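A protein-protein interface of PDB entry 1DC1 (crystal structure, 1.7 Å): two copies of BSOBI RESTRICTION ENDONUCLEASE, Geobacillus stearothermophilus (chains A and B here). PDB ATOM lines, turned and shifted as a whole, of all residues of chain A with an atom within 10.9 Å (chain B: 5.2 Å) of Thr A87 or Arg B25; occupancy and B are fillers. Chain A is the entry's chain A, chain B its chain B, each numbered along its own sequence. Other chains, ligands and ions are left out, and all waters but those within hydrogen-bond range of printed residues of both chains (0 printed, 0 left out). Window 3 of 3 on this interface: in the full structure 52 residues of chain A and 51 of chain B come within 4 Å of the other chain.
The side-chain hydroxyl (OG) of Ser A79 sits close to the backbone NH (N) of Lys A81.
The side-chain hydroxyl of Ser A79 is in hydrogen-bond range of the backbone NH of Ala A82 (3.0 Å).
NZ of Lys A84 is in hydrogen-bond range of O of Lys A81, 2.9 Å away.
The side-chain hydroxyl of Thr A87 lies close to the backbone NH of Asp A89, at 3.4 Å.
The side-chain carboxylate of Asp A90 lies within hydrogen-bond range of the backbone NH of Thr A87.
NH1 of Arg B25 is in salt-bridge range of OE1 of Glu B22 (3.1 Å).
The guanidinium group (NE) of Arg B25 lies within salt-bridge range of the side-chain carboxylate (OD2) of Asp A90, 2.7 Å away.
Phe B28 touches Lys A81.
Ala A82 touches Phe B28.
Lys A84 touches Tyr B21 (O to OH, 3.9 Å).
OH of Tyr B21 touches CA of Phe A85, 3.6 Å away.
Phe A85 touches Arg B25 (O to CD, 3.1 Å).
Phe B28 touches Phe A85 (CE2 to CD1, 3.4 Å).
Ile B29 touches Leu A86.
Arg B25 touches Thr A87.
Asp A90 touches Ile B29.
Printed residues of chain B within 4 Å of Ala A82: Phe B28.
Printed residues of chain B within 4 Å of Leu A86: Ile B29 (3.6 Å).
Printed residues of chain B within 4 Å of Thr A87: Arg B25 (3.9 Å).
Ser A94 touches none of the printed residues of chain B.
Of chain A, only Lys A84 (3.9 Å) and Phe A85 (3.6 Å) come within 4 Å of Tyr B21.
Of the printed residues of chain A, Arg B25 touches Phe A85, Thr A87 and Asp A90.
No residue of chain A comes within 4 Å of Ala B26.
No residue of chain A comes within 4 Å of Gly B27.
Ile B29 touches two residues of chain A.
The nearest printed residue of chain A that does not touch Arg B25 is Leu A86 (4.7 Å).
No position is printed for both chains.
Of the 10 pairs that touch across the chains among the printed residues, none has its exchanged pair printed and touching as well.
Of the 10 printed residues of chain B, 4 touch a printed residue of chain A.
Hydrophobic or aromatic side chains of chain A that line the printed part of chain B: Ala A82, Phe A85 and Leu A86.
Along chain A the printed residues that touch a printed residue of chain B span positions 81 to 90.
Among the printed residues, 10 pairs touch across the chains.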
ATOM      1  N   LEU A  73      30.196 -20.958  19.491  1.00  0.00           N
ATOM      2  CA  LEU A  73      30.115 -19.526  19.264  1.00  0.00           C
ATOM      3  C   LEU A  73      31.480 -19.055  18.802  1.00  0.00           C
ATOM      4  O   LEU A  73      31.598 -18.288  17.838  1.00  0.00           O
ATOM      5  CB  LEU A  73      29.738 -18.788  20.559  1.00  0.00           C
ATOM      6  CG  LEU A  73      29.575 -17.266  20.346  1.00  0.00           C
ATOM      7  CD1 LEU A  73      28.575 -16.949  19.207  1.00  0.00           C
ATOM      8  CD2 LEU A  73      29.137 -16.644  21.650  1.00  0.00           C
ATOM      9  N   SER A  76      32.238 -20.026  15.328  1.00  0.00           N
ATOM     10  CA  SER A  76      31.365 -19.284  14.432  1.00  0.00           C
ATOM     11  C   SER A  76      31.957 -17.899  14.081  1.00  0.00           C
ATOM     12  O   SER A  76      31.327 -17.119  13.365  1.00  0.00           O
ATOM     13  CB  SER A  76      29.921 -19.204  15.038  1.00  0.00           C
ATOM     14  OG  SER A  76      29.755 -18.181  16.008  1.00  0.00           O
ATOM     15  N   ILE A  78      33.247 -15.521  16.440  1.00  0.00           N
ATOM     16  CA  ILE A  78      33.052 -14.520  17.510  1.00  0.00           C
ATOM     17  C   ILE A  78      34.152 -14.581  18.596  1.00  0.00           C
ATOM     18  O   ILE A  78      34.233 -15.536  19.399  1.00  0.00           O
ATOM     19  CB  ILE A  78      31.621 -14.643  18.244  1.00  0.00           C
ATOM     20  CG1 ILE A  78      30.451 -14.496  17.245  1.00  0.00           C
ATOM     21  CG2 ILE A  78      31.458 -13.543  19.291  1.00  0.00           C
ATOM     22  CD1 ILE A  78      30.583 -13.346  16.229  1.00  0.00           C
ATOM     23  N   SER A  79      35.007 -13.561  18.599  1.00  0.00           N
ATOM     24  CA  SER A  79      36.068 -13.478  19.604  1.00  0.00           C
ATOM     25  C   SER A  79      35.396 -13.162  20.963  1.00  0.00           C
ATOM     26  O   SER A  79      34.238 -12.717  21.004  1.00  0.00           O
ATOM     27  CB  SER A  79      37.048 -12.357  19.235  1.00  0.00           C
ATOM     28  OG  SER A  79      36.418 -11.110  19.421  1.00  0.00           O
ATOM     29  N   LYS A  81      36.133 -10.804  22.816  1.00  0.00           N
ATOM     30  CA  LYS A  81      36.008  -9.359  22.857  1.00  0.00           C
ATOM     31  C   LYS A  81      34.711  -8.947  22.144  1.00  0.00           C
ATOM     32  O   LYS A  81      33.958  -8.151  22.684  1.00  0.00           O
ATOM     33  CB  LYS A  81      37.240  -8.728  22.200  1.00  0.00           C
ATOM     34  CG  LYS A  81      37.033  -7.355  21.651  1.00  0.00           C
ATOM     35  CD  LYS A  81      38.415  -6.686  21.369  1.00  0.00           C
ATOM     36  CE  LYS A  81      39.138  -6.231  22.675  1.00  0.00           C
ATOM     37  NZ  LYS A  81      40.409  -5.421  22.418  1.00  0.00           N
ATOM     38  N   ALA A  82      34.431  -9.509  20.966  1.00  0.00           N
ATOM     39  CA  ALA A  82      33.219  -9.184  20.211  1.00  0.00           C
ATOM     40  C   ALA A  82      31.962  -9.673  20.951  1.00  0.00           C
ATOM     41  O   ALA A  82      30.912  -9.060  20.881  1.00  0.00           O
ATOM     42  CB  ALA A  82      33.277  -9.850  18.835  1.00  0.00           C
ATOM     43  N   LYS A  83      32.099 -10.795  21.650  1.00  0.00           N
ATOM     44  CA  LYS A  83      31.002 -11.452  22.339  1.00  0.00           C
ATOM     45  C   LYS A  83      30.282 -10.510  23.304  1.00  0.00           C
ATOM     46  O   LYS A  83      29.053 -10.538  23.453  1.00  0.00           O
ATOM     47  CB  LYS A  83      31.556 -12.701  23.059  1.00  0.00           C
ATOM     48  CG  LYS A  83      30.527 -13.405  23.875  1.00  0.00           C
ATOM     49  CD  LYS A  83      31.009 -14.760  24.099  1.00  0.00           C
ATOM     50  CE  LYS A  83      31.598 -14.891  25.445  1.00  0.00           C
ATOM     51  NZ  LYS A  83      31.530 -16.357  25.830  1.00  0.00           N
ATOM     52  N   LYS A  84      31.061  -9.644  23.925  1.00  0.00           N
ATOM     53  CA  LYS A  84      30.531  -8.681  24.859  1.00  0.00           C
ATOM     54  C   LYS A  84      29.425  -7.773  24.299  1.00  0.00           C
ATOM     55  O   LYS A  84      28.573  -7.310  25.067  1.00  0.00           O
ATOM     56  CB  LYS A  84      31.656  -7.771  25.332  1.00  0.00           C
ATOM     57  CG  LYS A  84      32.752  -8.409  26.127  1.00  0.00           C
ATOM     58  CD  LYS A  84      33.764  -7.337  26.657  1.00  0.00           C
ATOM     59  CE  LYS A  84      33.990  -6.087  25.695  1.00  0.00           C
ATOM     60  NZ  LYS A  84      35.042  -6.227  24.609  1.00  0.00           N
ATOM     61  N   PHE A  85      29.452  -7.514  22.987  1.00  0.00           N
ATOM     62  CA  PHE A  85      28.477  -6.602  22.350  1.00  0.00           C
ATOM     63  C   PHE A  85      27.279  -7.307  21.666  1.00  0.00           C
ATOM     64  O   PHE A  85      26.372  -6.661  21.160  1.00  0.00           O
ATOM     65  CB  PHE A  85      29.229  -5.645  21.372  1.00  0.00           C
ATOM     66  CG  PHE A  85      30.291  -4.785  22.037  1.00  0.00           C
ATOM     67  CD1 PHE A  85      31.576  -5.279  22.249  1.00  0.00           C
ATOM     68  CD2 PHE A  85      29.974  -3.526  22.524  1.00  0.00           C
ATOM     69  CE1 PHE A  85      32.497  -4.534  22.948  1.00  0.00           C
ATOM     70  CE2 PHE A  85      30.908  -2.772  23.229  1.00  0.00           C
ATOM     71  CZ  PHE A  85      32.160  -3.270  23.447  1.00  0.00           C
ATOM     72  N   LEU A  86      27.268  -8.636  21.718  1.00  0.00           N
ATOM     73  CA  LEU A  86      26.217  -9.426  21.096  1.00  0.00           C
ATOM     74  C   LEU A  86      25.066  -9.792  22.034  1.00  0.00           C
ATOM     75  O   LEU A  86      25.296 -10.133  23.177  1.00  0.00           O
ATOM     76  CB  LEU A  86      26.813 -10.735  20.587  1.00  0.00           C
ATOM     77  CG  LEU A  86      27.957 -10.674  19.575  1.00  0.00           C
ATOM     78  CD1 LEU A  86      28.113 -12.056  18.980  1.00  0.00           C
ATOM     79  CD2 LEU A  86      27.719  -9.594  18.485  1.00  0.00           C
ATOM     80  N   THR A  87      23.842  -9.774  21.531  1.00  0.00           N
ATOM     81  CA  THR A  87      22.688 -10.197  22.313  1.00  0.00           C
ATOM     82  C   THR A  87      22.644 -11.726  22.176  1.00  0.00           C
ATOM     83  O   THR A  87      23.352 -12.317  21.349  1.00  0.00           O
ATOM     84  CB  THR A  87      21.389  -9.677  21.738  1.00  0.00           C
ATOM     85  OG1 THR A  87      21.213 -10.255  20.438  1.00  0.00           O
ATOM     86  CG2 THR A  87      21.414  -8.166  21.612  1.00  0.00           C
ATOM     87  N   GLU A  88      21.823 -12.383  22.975  1.00  0.00           N
ATOM     88  CA  GLU A  88      21.739 -13.835  22.875  1.00  0.00           C
ATOM     89  C   GLU A  88      21.311 -14.280  21.470  1.00  0.00           C
ATOM     90  O   GLU A  88      21.793 -15.283  20.961  1.00  0.00           O
ATOM     91  CB  GLU A  88      20.777 -14.417  23.930  1.00  0.00           C
ATOM     92  CG  GLU A  88      21.295 -14.365  25.371  1.00  0.00           C
ATOM     93  CD  GLU A  88      22.752 -14.889  25.523  1.00  0.00           C
ATOM     94  OE1 GLU A  88      22.976 -16.111  25.637  1.00  0.00           O
ATOM     95  OE2 GLU A  88      23.684 -14.064  25.531  1.00  0.00           O
ATOM     96  N   ASP A  89      20.415 -13.524  20.853  1.00  0.00           N
ATOM     97  CA  ASP A  89      19.914 -13.811  19.507  1.00  0.00           C
ATOM     98  C   ASP A  89      21.031 -13.681  18.453  1.00  0.00           C
ATOM     99  O   ASP A  89      21.054 -14.446  17.462  1.00  0.00           O
ATOM    100  CB  ASP A  89      18.771 -12.843  19.189  1.00  0.00           C
ATOM    101  CG  ASP A  89      17.454 -13.273  19.789  1.00  0.00           C
ATOM    102  OD1 ASP A  89      17.364 -14.365  20.376  1.00  0.00           O
ATOM    103  OD2 ASP A  89      16.494 -12.509  19.656  1.00  0.00           O
ATOM    104  N   ASP A  90      21.930 -12.696  18.664  1.00  0.00           N
ATOM    105  CA  ASP A  90      23.070 -12.453  17.761  1.00  0.00           C
ATOM    106  C   ASP A  90      23.921 -13.707  17.779  1.00  0.00           C
ATOM    107  O   ASP A  90      24.322 -14.244  16.752  1.00  0.00           O
ATOM    108  CB  ASP A  90      23.928 -11.305  18.274  1.00  0.00           C
ATOM    109  CG  ASP A  90      23.339  -9.937  17.967  1.00  0.00           C
ATOM    110  OD1 ASP A  90      22.524  -9.766  17.047  1.00  0.00           O
ATOM    111  OD2 ASP A  90      23.702  -8.984  18.668  1.00  0.00           O
ATOM    112  N   LYS A  91      24.191 -14.172  18.981  1.00  0.00           N
ATOM    113  CA  LYS A  91      24.982 -15.364  19.173  1.00  0.00           C
ATOM    114  C   LYS A  91      24.363 -16.599  18.519  1.00  0.00           C
ATOM    115  O   LYS A  91      25.054 -17.363  17.860  1.00  0.00           O
ATOM    116  CB  LYS A  91      25.172 -15.618  20.660  1.00  0.00           C
ATOM    117  CG  LYS A  91      25.878 -14.522  21.338  1.00  0.00           C
ATOM    118  CD  LYS A  91      25.908 -14.828  22.815  1.00  0.00           C
ATOM    119  CE  LYS A  91      26.524 -13.675  23.542  1.00  0.00           C
ATOM    120  NZ  LYS A  91      26.545 -13.917  25.014  1.00  0.00           N
ATOM    121  N   LYS A  92      23.065 -16.815  18.760  1.00  0.00           N
ATOM    122  CA  LYS A  92      22.267 -17.936  18.205  1.00  0.00           C
ATOM    123  C   LYS A  92      22.419 -17.887  16.714  1.00  0.00           C
ATOM    124  O   LYS A  92      22.653 -18.881  16.048  1.00  0.00           O
ATOM    125  CB  LYS A  92      20.753 -17.720  18.492  1.00  0.00           C
ATOM    126  CG  LYS A  92      20.080 -18.758  19.333  1.00  0.00           C
ATOM    127  CD  LYS A  92      19.315 -18.132  20.503  1.00  0.00           C
ATOM    128  CE  LYS A  92      19.903 -18.600  21.860  1.00  0.00           C
ATOM    129  NZ  LYS A  92      18.908 -18.880  22.959  1.00  0.00           N
ATOM    130  N   GLU A  93      22.249 -16.684  16.197  1.00  0.00           N
ATOM    131  CA  GLU A  93      22.330 -16.447  14.777  1.00  0.00           C
ATOM    132  C   GLU A  93      23.720 -16.798  14.226  1.00  0.00           C
ATOM    133  O   GLU A  93      23.842 -17.433  13.172  1.00  0.00           O
ATOM    134  CB  GLU A  93      22.020 -14.984  14.530  1.00  0.00           C
ATOM    135  CG  GLU A  93      21.325 -14.696  13.223  1.00  0.00           C
ATOM    136  CD  GLU A  93      21.561 -13.270  12.797  1.00  0.00           C
ATOM    137  OE1 GLU A  93      21.218 -12.342  13.589  1.00  0.00           O
ATOM    138  OE2 GLU A  93      22.106 -13.090  11.683  1.00  0.00           O
ATOM    139  N   SER A  94      24.761 -16.370  14.937  1.00  0.00           N
ATOM    140  CA  SER A  94      26.127 -16.667  14.535  1.00  0.00           C
ATOM    141  C   SER A  94      26.348 -18.182  14.485  1.00  0.00           C
ATOM    142  O   SER A  94      26.923 -18.698  13.551  1.00  0.00           O
ATOM    143  CB  SER A  94      27.126 -16.025  15.515  1.00  0.00           C
ATOM    144  OG  SER A  94      28.422 -15.971  14.921  1.00  0.00           O
ATOM    145  N   ILE A  95      25.877 -18.883  15.496  1.00  0.00           N
ATOM    146  CA  ILE A  95      26.054 -20.296  15.516  1.00  0.00           C
ATOM    147  C   ILE A  95      25.282 -20.939  14.358  1.00  0.00           C
ATOM    148  O   ILE A  95      25.782 -21.875  13.726  1.00  0.00           O
ATOM    149  CB  ILE A  95      25.641 -20.863  16.850  1.00  0.00           C
ATOM    150  CG1 ILE A  95      26.725 -20.523  17.866  1.00  0.00           C
ATOM    151  CG2 ILE A  95      25.549 -22.387  16.761  1.00  0.00           C
ATOM    152  CD1 ILE A  95      26.273 -20.639  19.315  1.00  0.00           C
ATOM    153  N   TYR B  21      26.699   2.769  21.532  1.00  0.00           N
ATOM    154  CA  TYR B  21      26.696   1.349  21.801  1.00  0.00           C
ATOM    155  C   TYR B  21      26.186   0.550  20.566  1.00  0.00           C
ATOM    156  O   TYR B  21      26.778  -0.468  20.176  1.00  0.00           O
ATOM    157  CB  TYR B  21      25.830   1.111  23.032  1.00  0.00           C
ATOM    158  CG  TYR B  21      25.849  -0.328  23.405  1.00  0.00           C
ATOM    159  CD1 TYR B  21      26.922  -0.865  24.098  1.00  0.00           C
ATOM    160  CD2 TYR B  21      24.866  -1.185  22.942  1.00  0.00           C
ATOM    161  CE1 TYR B  21      27.027  -2.231  24.317  1.00  0.00           C
ATOM    162  CE2 TYR B  21      24.959  -2.564  23.155  1.00  0.00           C
ATOM    163  CZ  TYR B  21      26.041  -3.068  23.838  1.00  0.00           C
ATOM    164  OH  TYR B  21      26.130  -4.423  24.024  1.00  0.00           O
ATOM    165  N   GLU B  22      25.123   1.026  19.925  1.00  0.00           N
ATOM    166  CA  GLU B  22      24.625   0.302  18.768  1.00  0.00           C
ATOM    167  C   GLU B  22      25.584   0.273  17.581  1.00  0.00           C
ATOM    168  O   GLU B  22      25.634  -0.734  16.842  1.00  0.00           O
ATOM    169  CB  GLU B  22      23.268   0.862  18.356  1.00  0.00           C
ATOM    170  CG  GLU B  22      22.161   0.370  19.305  1.00  0.00           C
ATOM    171  CD  GLU B  22      22.138  -1.181  19.507  1.00  0.00           C
ATOM    172  OE1 GLU B  22      22.522  -1.944  18.580  1.00  0.00           O
ATOM    173  OE2 GLU B  22      21.726  -1.631  20.605  1.00  0.00           O
ATOM    174  N   GLU B  23      26.348   1.355  17.413  1.00  0.00           N
ATOM    175  CA  GLU B  23      27.311   1.432  16.341  1.00  0.00           C
ATOM    176  C   GLU B  23      28.459   0.443  16.622  1.00  0.00           C
ATOM    177  O   GLU B  23      28.988  -0.190  15.716  1.00  0.00           O
ATOM    178  CB  GLU B  23      27.820   2.866  16.201  1.00  0.00           C
ATOM    179  CG  GLU B  23      27.089   3.676  15.103  1.00  0.00           C
ATOM    180  CD  GLU B  23      26.359   2.805  14.017  1.00  0.00           C
ATOM    181  OE1 GLU B  23      27.043   2.297  13.095  1.00  0.00           O
ATOM    182  OE2 GLU B  23      25.100   2.630  14.088  1.00  0.00           O
ATOM    183  N   TYR B  24      28.841   0.322  17.888  1.00  0.00           N
ATOM    184  CA  TYR B  24      29.888  -0.633  18.273  1.00  0.00           C
ATOM    185  C   TYR B  24      29.410  -2.083  17.985  1.00  0.00           C
ATOM    186  O   TYR B  24      30.138  -2.863  17.371  1.00  0.00           O
ATOM    187  CB  TYR B  24      30.262  -0.482  19.773  1.00  0.00           C
ATOM    188  CG  TYR B  24      31.285   0.623  20.068  1.00  0.00           C
ATOM    189  CD1 TYR B  24      32.491   0.711  19.339  1.00  0.00           C
ATOM    190  CD2 TYR B  24      31.055   1.578  21.050  1.00  0.00           C
ATOM    191  CE1 TYR B  24      33.438   1.721  19.579  1.00  0.00           C
ATOM    192  CE2 TYR B  24      32.024   2.604  21.293  1.00  0.00           C
ATOM    193  CZ  TYR B  24      33.199   2.655  20.551  1.00  0.00           C
ATOM    194  OH  TYR B  24      34.134   3.615  20.782  1.00  0.00           O
ATOM    195  N   ARG B  25      28.211  -2.448  18.441  1.00  0.00           N
ATOM    196  CA  ARG B  25      27.687  -3.777  18.178  1.00  0.00           C
ATOM    197  C   ARG B  25      27.605  -4.024  16.660  1.00  0.00           C
ATOM    198  O   ARG B  25      28.041  -5.089  16.155  1.00  0.00           O
ATOM    199  CB  ARG B  25      26.326  -3.897  18.861  1.00  0.00           C
ATOM    200  CG  ARG B  25      25.573  -5.126  18.538  1.00  0.00           C
ATOM    201  CD  ARG B  25      24.310  -5.180  19.392  1.00  0.00           C
ATOM    202  NE  ARG B  25      23.487  -6.278  18.884  1.00  0.00           N
ATOM    203  CZ  ARG B  25      22.453  -6.125  18.063  1.00  0.00           C
ATOM    204  NH1 ARG B  25      22.113  -4.908  17.666  1.00  0.00           N
ATOM    205  NH2 ARG B  25      21.799  -7.181  17.582  1.00  0.00           N
ATOM    206  N   ALA B  26      27.070  -3.055  15.913  1.00  0.00           N
ATOM    207  CA  ALA B  26      26.990  -3.217  14.455  1.00  0.00           C
ATOM    208  C   ALA B  26      28.375  -3.481  13.848  1.00  0.00           C
ATOM    209  O   ALA B  26      28.504  -4.337  12.989  1.00  0.00           O
ATOM    210  CB  ALA B  26      26.373  -1.967  13.827  1.00  0.00           C
ATOM    211  N   GLY B  27      29.397  -2.741  14.294  1.00  0.00           N
ATOM    212  CA  GLY B  27      30.765  -2.896  13.784  1.00  0.00           C
ATOM    213  C   GLY B  27      31.342  -4.263  14.087  1.00  0.00           C
ATOM    214  O   GLY B  27      31.928  -4.931  13.227  1.00  0.00           O
ATOM    215  N   PHE B  28      31.163  -4.710  15.327  1.00  0.00           N
ATOM    216  CA  PHE B  28      31.652  -6.022  15.696  1.00  0.00           C
ATOM    217  C   PHE B  28      30.960  -7.100  14.854  1.00  0.00           C
ATOM    218  O   PHE B  28      31.616  -8.015  14.409  1.00  0.00           O
ATOM    219  CB  PHE B  28      31.466  -6.278  17.210  1.00  0.00           C
ATOM    220  CG  PHE B  28      32.635  -5.749  18.087  1.00  0.00           C
ATOM    221  CD1 PHE B  28      33.930  -6.311  18.000  1.00  0.00           C
ATOM    222  CD2 PHE B  28      32.447  -4.681  18.966  1.00  0.00           C
ATOM    223  CE1 PHE B  28      34.996  -5.822  18.762  1.00  0.00           C
ATOM    224  CE2 PHE B  28      33.522  -4.170  19.749  1.00  0.00           C
ATOM    225  CZ  PHE B  28      34.787  -4.738  19.643  1.00  0.00           C
ATOM    226  N   ILE B  29      29.650  -6.986  14.619  1.00  0.00           N
ATOM    227  CA  ILE B  29      28.940  -7.961  13.786  1.00  0.00           C
ATOM    228  C   ILE B  29      29.453  -7.994  12.316  1.00  0.00           C
ATOM    229  O   ILE B  29      29.674  -9.068  11.741  1.00  0.00           O
ATOM    230  CB  ILE B  29      27.438  -7.662  13.883  1.00  0.00           C
ATOM    231  CG1 ILE B  29      26.960  -8.069  15.278  1.00  0.00           C
ATOM    232  CG2 ILE B  29      26.660  -8.387  12.805  1.00  0.00           C
ATOM    233  CD1 ILE B  29      25.550  -7.593  15.604  1.00  0.00           C
ATOM    234  N   ALA B  30      29.663  -6.816  11.727  1.00  0.00           N
ATOM    235  CA  ALA B  30      30.179  -6.710  10.364  1.00  0.00           C
ATOM    236  C   ALA B  30      31.605  -7.250  10.289  1.00  0.00           C
ATOM    237  O   ALA B  30      31.970  -7.864   9.306  1.00  0.00           O
ATOM    238  CB  ALA B  30      30.143  -5.252   9.895  1.00  0.00           C
